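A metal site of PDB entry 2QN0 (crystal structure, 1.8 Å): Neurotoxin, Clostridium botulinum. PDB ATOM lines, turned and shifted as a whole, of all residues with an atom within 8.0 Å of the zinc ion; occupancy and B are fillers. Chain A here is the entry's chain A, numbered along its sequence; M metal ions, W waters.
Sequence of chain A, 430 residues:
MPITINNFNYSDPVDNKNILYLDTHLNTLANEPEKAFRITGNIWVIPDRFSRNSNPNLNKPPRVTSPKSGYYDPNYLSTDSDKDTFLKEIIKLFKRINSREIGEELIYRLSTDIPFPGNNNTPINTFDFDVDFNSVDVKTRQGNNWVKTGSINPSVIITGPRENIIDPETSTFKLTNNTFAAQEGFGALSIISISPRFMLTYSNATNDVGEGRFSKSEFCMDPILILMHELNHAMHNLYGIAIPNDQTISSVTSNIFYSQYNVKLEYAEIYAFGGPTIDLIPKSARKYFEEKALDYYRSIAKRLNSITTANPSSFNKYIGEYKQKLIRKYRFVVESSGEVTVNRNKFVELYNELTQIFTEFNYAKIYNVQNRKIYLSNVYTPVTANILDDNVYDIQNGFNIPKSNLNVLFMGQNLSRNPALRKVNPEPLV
The zinc ion is bound by the side-chain carboxylate of Glu 269, water W1, a ring nitrogen (NE2) of His 233 and a ring nitrogen (NE2) of His 229. Slightly farther from the zinc ion lies OE2 of Glu 269 (2.7 Å).
The side-chain carboxylate of Glu 360 is in hydrogen-bond range of a ring nitrogen (ND1) of His 229 (2.7 Å). OG1 of Thr 170 is in hydrogen-bond range of OE1 of Glu 230 (2.6 Å). OH of Tyr 375 sits close to OE1 of Glu 269 (3.3 Å).
Merely in contact with the zinc ion: Glu 230. Within 4 Å of the zinc ion: His 229, Glu 230, His 233 and Glu 269. The nearest printed residue that does not touch the zinc ion is Tyr 375 (4.2 Å).
Water W1 bridges the side-chain carboxylate of Glu 230 and the side-chain carboxylate of Glu 269.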
ATOM      1  N   ASP A 167     -23.403 -33.083  12.337  1.00  0.00           N
ATOM      2  CA  ASP A 167     -24.393 -32.016  12.231  1.00  0.00           C
ATOM      3  C   ASP A 167     -23.681 -30.708  11.883  1.00  0.00           C
ATOM      4  O   ASP A 167     -23.549 -29.818  12.721  1.00  0.00           O
ATOM      5  CB  ASP A 167     -25.174 -31.871  13.539  1.00  0.00           C
ATOM      6  CG  ASP A 167     -26.314 -30.879  13.440  1.00  0.00           C
ATOM      7  OD1 ASP A 167     -26.839 -30.677  12.321  1.00  0.00           O
ATOM      8  OD2 ASP A 167     -26.699 -30.292  14.478  1.00  0.00           O
ATOM      9  N   PRO A 168     -23.171 -30.602  10.645  1.00  0.00           N
ATOM     10  CA  PRO A 168     -22.471 -29.391  10.221  1.00  0.00           C
ATOM     11  C   PRO A 168     -23.358 -28.178  10.468  1.00  0.00           C
ATOM     12  O   PRO A 168     -24.579 -28.239  10.323  1.00  0.00           O
ATOM     13  CB  PRO A 168     -22.208 -29.645   8.742  1.00  0.00           C
ATOM     14  CG  PRO A 168     -23.285 -30.597   8.344  1.00  0.00           C
ATOM     15  CD  PRO A 168     -23.359 -31.530   9.518  1.00  0.00           C
ATOM     16  N   GLU A 169     -22.739 -27.062  10.855  1.00  0.00           N
ATOM     17  CA  GLU A 169     -23.501 -25.860  11.183  1.00  0.00           C
ATOM     18  C   GLU A 169     -22.771 -24.560  10.846  1.00  0.00           C
ATOM     19  O   GLU A 169     -21.570 -24.428  11.077  1.00  0.00           O
ATOM     20  CB  GLU A 169     -23.828 -25.921  12.678  1.00  0.00           C
ATOM     21  CG  GLU A 169     -24.319 -24.657  13.324  1.00  0.00           C
ATOM     22  CD  GLU A 169     -24.825 -24.910  14.734  1.00  0.00           C
ATOM     23  OE1 GLU A 169     -24.378 -25.889  15.365  1.00  0.00           O
ATOM     24  OE2 GLU A 169     -25.674 -24.132  15.212  1.00  0.00           O
ATOM     25  N   THR A 170     -23.520 -23.607  10.293  1.00  0.00           N
ATOM     26  CA  THR A 170     -22.977 -22.300   9.922  1.00  0.00           C
ATOM     27  C   THR A 170     -23.713 -21.263  10.770  1.00  0.00           C
ATOM     28  O   THR A 170     -24.941 -21.304  10.859  1.00  0.00           O
ATOM     29  CB  THR A 170     -23.219 -21.980   8.447  1.00  0.00           C
ATOM     30  OG1 THR A 170     -22.561 -22.955   7.629  1.00  0.00           O
ATOM     31  CG2 THR A 170     -22.698 -20.586   8.103  1.00  0.00           C
ATOM     32  N   ILE A 226     -21.444 -31.469   0.917  1.00  0.00           N
ATOM     33  CA  ILE A 226     -21.690 -31.225   2.332  1.00  0.00           C
ATOM     34  C   ILE A 226     -21.115 -29.853   2.664  1.00  0.00           C
ATOM     35  O   ILE A 226     -21.735 -29.040   3.349  1.00  0.00           O
ATOM     36  CB  ILE A 226     -21.009 -32.310   3.202  1.00  0.00           C
ATOM     37  CG1 ILE A 226     -21.596 -33.684   2.878  1.00  0.00           C
ATOM     38  CG2 ILE A 226     -21.191 -31.985   4.676  1.00  0.00           C
ATOM     39  CD1 ILE A 226     -20.964 -34.837   3.653  1.00  0.00           C
ATOM     40  N   HIS A 229     -22.876 -26.920   0.650  1.00  0.00           N
ATOM     41  CA  HIS A 229     -24.178 -26.629   1.247  1.00  0.00           C
ATOM     42  C   HIS A 229     -23.990 -25.557   2.326  1.00  0.00           C
ATOM     43  O   HIS A 229     -24.743 -24.583   2.370  1.00  0.00           O
ATOM     44  CB  HIS A 229     -24.782 -27.900   1.869  1.00  0.00           C
ATOM     45  CG  HIS A 229     -26.024 -27.649   2.657  1.00  0.00           C
ATOM     46  ND1 HIS A 229     -27.282 -27.968   2.172  1.00  0.00           N
ATOM     47  CD2 HIS A 229     -26.216 -27.114   3.882  1.00  0.00           C
ATOM     48  CE1 HIS A 229     -28.191 -27.633   3.080  1.00  0.00           C
ATOM     49  NE2 HIS A 229     -27.570 -27.115   4.123  1.00  0.00           N
ATOM     50  N   GLU A 230     -22.982 -25.721   3.180  1.00  0.00           N
ATOM     51  CA  GLU A 230     -22.731 -24.741   4.225  1.00  0.00           C
ATOM     52  C   GLU A 230     -22.240 -23.429   3.618  1.00  0.00           C
ATOM     53  O   GLU A 230     -22.542 -22.347   4.138  1.00  0.00           O
ATOM     54  CB  GLU A 230     -21.710 -25.260   5.248  1.00  0.00           C
ATOM     55  CG  GLU A 230     -22.168 -26.473   6.068  1.00  0.00           C
ATOM     56  CD  GLU A 230     -23.541 -26.308   6.707  1.00  0.00           C
ATOM     57  OE1 GLU A 230     -23.830 -25.226   7.280  1.00  0.00           O
ATOM     58  OE2 GLU A 230     -24.343 -27.256   6.642  1.00  0.00           O
ATOM     59  N   LEU A 231     -21.482 -23.501   2.525  1.00  0.00           N
ATOM     60  CA  LEU A 231     -21.008 -22.279   1.883  1.00  0.00           C
ATOM     61  C   LEU A 231     -22.210 -21.471   1.370  1.00  0.00           C
ATOM     62  O   LEU A 231     -22.134 -20.248   1.236  1.00  0.00           O
ATOM     63  CB  LEU A 231     -20.048 -22.607   0.723  1.00  0.00           C
ATOM     64  CG  LEU A 231     -18.707 -23.232   1.135  1.00  0.00           C
ATOM     65  CD1 LEU A 231     -17.859 -23.487  -0.122  1.00  0.00           C
ATOM     66  CD2 LEU A 231     -17.966 -22.311   2.091  1.00  0.00           C
ATOM     67  N   ASN A 232     -23.315 -22.143   1.098  1.00  0.00           N
ATOM     68  CA  ASN A 232     -24.513 -21.438   0.648  1.00  0.00           C
ATOM     69  C   ASN A 232     -25.075 -20.622   1.794  1.00  0.00           C
ATOM     70  O   ASN A 232     -25.538 -19.498   1.607  1.00  0.00           O
ATOM     71  CB  ASN A 232     -25.568 -22.417   0.116  1.00  0.00           C
ATOM     72  CG  ASN A 232     -25.151 -23.054  -1.191  1.00  0.00           C
ATOM     73  OD1 ASN A 232     -24.287 -22.533  -1.900  1.00  0.00           O
ATOM     74  ND2 ASN A 232     -25.767 -24.185  -1.518  1.00  0.00           N
ATOM     75  N   HIS A 233     -25.053 -21.189   3.008  1.00  0.00           N
ATOM     76  CA  HIS A 233     -25.529 -20.434   4.171  1.00  0.00           C
ATOM     77  C   HIS A 233     -24.618 -19.211   4.319  1.00  0.00           C
ATOM     78  O   HIS A 233     -25.084 -18.112   4.612  1.00  0.00           O
ATOM     79  CB  HIS A 233     -25.464 -21.272   5.437  1.00  0.00           C
ATOM     80  CG  HIS A 233     -26.520 -22.325   5.518  1.00  0.00           C
ATOM     81  ND1 HIS A 233     -27.864 -22.038   5.389  1.00  0.00           N
ATOM     82  CD2 HIS A 233     -26.446 -23.660   5.741  1.00  0.00           C
ATOM     83  CE1 HIS A 233     -28.567 -23.156   5.534  1.00  0.00           C
ATOM     84  NE2 HIS A 233     -27.725 -24.150   5.748  1.00  0.00           N
ATOM     85  N   GLU A 266     -36.425 -25.383   8.366  1.00  0.00           N
ATOM     86  CA  GLU A 266     -36.157 -23.955   8.207  1.00  0.00           C
ATOM     87  C   GLU A 266     -36.104 -23.545   6.742  1.00  0.00           C
ATOM     88  O   GLU A 266     -35.587 -24.281   5.891  1.00  0.00           O
ATOM     89  CB  GLU A 266     -34.828 -23.587   8.870  1.00  0.00           C
ATOM     90  CG  GLU A 266     -34.738 -23.979  10.327  1.00  0.00           C
ATOM     91  CD  GLU A 266     -33.425 -23.569  10.944  1.00  0.00           C
ATOM     92  OE1 GLU A 266     -32.391 -23.641  10.245  1.00  0.00           O
ATOM     93  OE2 GLU A 266     -33.405 -23.172  12.132  1.00  0.00           O
ATOM     94  N   ALA A 268     -34.286 -21.406   5.596  1.00  0.00           N
ATOM     95  CA  ALA A 268     -32.861 -21.211   5.295  1.00  0.00           C
ATOM     96  C   ALA A 268     -32.297 -22.492   4.694  1.00  0.00           C
ATOM     97  O   ALA A 268     -31.455 -22.459   3.787  1.00  0.00           O
ATOM     98  CB  ALA A 268     -32.111 -20.857   6.577  1.00  0.00           C
ATOM     99  N   GLU A 269     -32.750 -23.642   5.200  1.00  0.00           N
ATOM    100  CA  GLU A 269     -32.299 -24.938   4.696  1.00  0.00           C
ATOM    101  C   GLU A 269     -32.857 -25.183   3.303  1.00  0.00           C
ATOM    102  O   GLU A 269     -32.170 -25.711   2.432  1.00  0.00           O
ATOM    103  CB  GLU A 269     -32.748 -26.061   5.632  1.00  0.00           C
ATOM    104  CG  GLU A 269     -32.100 -26.030   7.010  1.00  0.00           C
ATOM    105  CD  GLU A 269     -30.590 -26.134   6.916  1.00  0.00           C
ATOM    106  OE1 GLU A 269     -30.096 -26.470   5.834  1.00  0.00           O
ATOM    107  OE2 GLU A 269     -29.909 -25.888   7.936  1.00  0.00           O
ATOM    108  N   ILE A 270     -34.112 -24.794   3.104  1.00  0.00           N
ATOM    109  CA  ILE A 270     -34.758 -24.981   1.811  1.00  0.00           C
ATOM    110  C   ILE A 270     -33.985 -24.227   0.715  1.00  0.00           C
ATOM    111  O   ILE A 270     -33.797 -24.747  -0.380  1.00  0.00           O
ATOM    112  CB  ILE A 270     -36.227 -24.509   1.860  1.00  0.00           C
ATOM    113  CG1 ILE A 270     -37.043 -25.469   2.740  1.00  0.00           C
ATOM    114  CG2 ILE A 270     -36.814 -24.444   0.445  1.00  0.00           C
ATOM    115  CD1 ILE A 270     -38.520 -25.110   2.871  1.00  0.00           C
ATOM    116  N   TYR A 271     -33.545 -23.009   1.008  1.00  0.00           N
ATOM    117  CA  TYR A 271     -32.792 -22.251   0.017  1.00  0.00           C
ATOM    118  C   TYR A 271     -31.391 -22.804  -0.190  1.00  0.00           C
ATOM    119  O   TYR A 271     -30.907 -22.862  -1.313  1.00  0.00           O
ATOM    120  CB  TYR A 271     -32.721 -20.772   0.406  1.00  0.00           C
ATOM    121  CG  TYR A 271     -33.937 -19.981  -0.048  1.00  0.00           C
ATOM    122  CD1 TYR A 271     -34.447 -20.131  -1.341  1.00  0.00           C
ATOM    123  CD2 TYR A 271     -34.543 -19.065   0.801  1.00  0.00           C
ATOM    124  CE1 TYR A 271     -35.544 -19.385  -1.776  1.00  0.00           C
ATOM    125  CE2 TYR A 271     -35.646 -18.313   0.371  1.00  0.00           C
ATOM    126  CZ  TYR A 271     -36.137 -18.470  -0.912  1.00  0.00           C
ATOM    127  OH  TYR A 271     -37.205 -17.711  -1.330  1.00  0.00           O
ATOM    128  N   ALA A 272     -30.741 -23.223   0.899  1.00  0.00           N
ATOM    129  CA  ALA A 272     -29.395 -23.780   0.784  1.00  0.00           C
ATOM    130  C   ALA A 272     -29.417 -25.056  -0.063  1.00  0.00           C
ATOM    131  O   ALA A 272     -28.493 -25.315  -0.849  1.00  0.00           O
ATOM    132  CB  ALA A 272     -28.839 -24.073   2.173  1.00  0.00           C
ATOM    133  N   PHE A 273     -30.467 -25.847   0.091  1.00  0.00           N
ATOM    134  CA  PHE A 273     -30.601 -27.085  -0.680  1.00  0.00           C
ATOM    135  C   PHE A 273     -31.056 -26.759  -2.105  1.00  0.00           C
ATOM    136  O   PHE A 273     -30.441 -27.204  -3.076  1.00  0.00           O
ATOM    137  CB  PHE A 273     -31.597 -28.044  -0.029  1.00  0.00           C
ATOM    138  CG  PHE A 273     -31.681 -29.369  -0.720  1.00  0.00           C
ATOM    139  CD1 PHE A 273     -30.648 -30.302  -0.583  1.00  0.00           C
ATOM    140  CD2 PHE A 273     -32.736 -29.661  -1.572  1.00  0.00           C
ATOM    141  CE1 PHE A 273     -30.678 -31.507  -1.291  1.00  0.00           C
ATOM    142  CE2 PHE A 273     -32.778 -30.858  -2.282  1.00  0.00           C
ATOM    143  CZ  PHE A 273     -31.745 -31.792  -2.145  1.00  0.00           C
ATOM    144  N   GLU A 360     -27.283 -26.526  -3.327  1.00  0.00           N
ATOM    145  CA  GLU A 360     -26.766 -27.894  -3.295  1.00  0.00           C
ATOM    146  C   GLU A 360     -27.323 -28.712  -4.457  1.00  0.00           C
ATOM    147  O   GLU A 360     -26.588 -29.437  -5.146  1.00  0.00           O
ATOM    148  CB  GLU A 360     -27.152 -28.562  -1.982  1.00  0.00           C
ATOM    149  CG  GLU A 360     -26.588 -29.964  -1.800  1.00  0.00           C
ATOM    150  CD  GLU A 360     -27.170 -30.667  -0.580  1.00  0.00           C
ATOM    151  OE1 GLU A 360     -27.360 -29.995   0.456  1.00  0.00           O
ATOM    152  OE2 GLU A 360     -27.426 -31.884  -0.661  1.00  0.00           O
ATOM    153  N   ARG A 372     -28.663 -36.731  -2.512  1.00  0.00           N
ATOM    154  CA  ARG A 372     -29.997 -36.900  -1.963  1.00  0.00           C
ATOM    155  C   ARG A 372     -30.964 -36.106  -2.834  1.00  0.00           C
ATOM    156  O   ARG A 372     -30.632 -35.038  -3.332  1.00  0.00           O
ATOM    157  CB  ARG A 372     -30.036 -36.403  -0.517  1.00  0.00           C
ATOM    158  CG  ARG A 372     -29.496 -34.984  -0.317  1.00  0.00           C
ATOM    159  CD  ARG A 372     -29.425 -34.629   1.169  1.00  0.00           C
ATOM    160  NE  ARG A 372     -28.771 -33.336   1.395  1.00  0.00           N
ATOM    161  CZ  ARG A 372     -28.509 -32.838   2.598  1.00  0.00           C
ATOM    162  NH1 ARG A 372     -28.848 -33.510   3.686  1.00  0.00           N
ATOM    163  NH2 ARG A 372     -27.909 -31.653   2.715  1.00  0.00           N
ATOM    164  N   TYR A 375     -33.690 -32.464   0.867  1.00  0.00           N
ATOM    165  CA  TYR A 375     -32.936 -32.192   2.074  1.00  0.00           C
ATOM    166  C   TYR A 375     -33.323 -33.159   3.193  1.00  0.00           C
ATOM    167  O   TYR A 375     -32.483 -33.591   3.984  1.00  0.00           O
ATOM    168  CB  TYR A 375     -33.185 -30.753   2.539  1.00  0.00           C
ATOM    169  CG  TYR A 375     -32.442 -30.389   3.802  1.00  0.00           C
ATOM    170  CD1 TYR A 375     -31.058 -30.238   3.806  1.00  0.00           C
ATOM    171  CD2 TYR A 375     -33.125 -30.199   5.002  1.00  0.00           C
ATOM    172  CE1 TYR A 375     -30.367 -29.914   4.979  1.00  0.00           C
ATOM    173  CE2 TYR A 375     -32.452 -29.862   6.177  1.00  0.00           C
ATOM    174  CZ  TYR A 375     -31.067 -29.721   6.155  1.00  0.00           C
ATOM    175  OH  TYR A 375     -30.394 -29.403   7.314  1.00  0.00           O
HETATM  176 ZN    ZN M   1     -28.046 -26.190   5.948  1.00  0.00          ZN
HETATM  177  O   HOH W   1     -26.788 -26.955   7.408  1.00  0.00           O
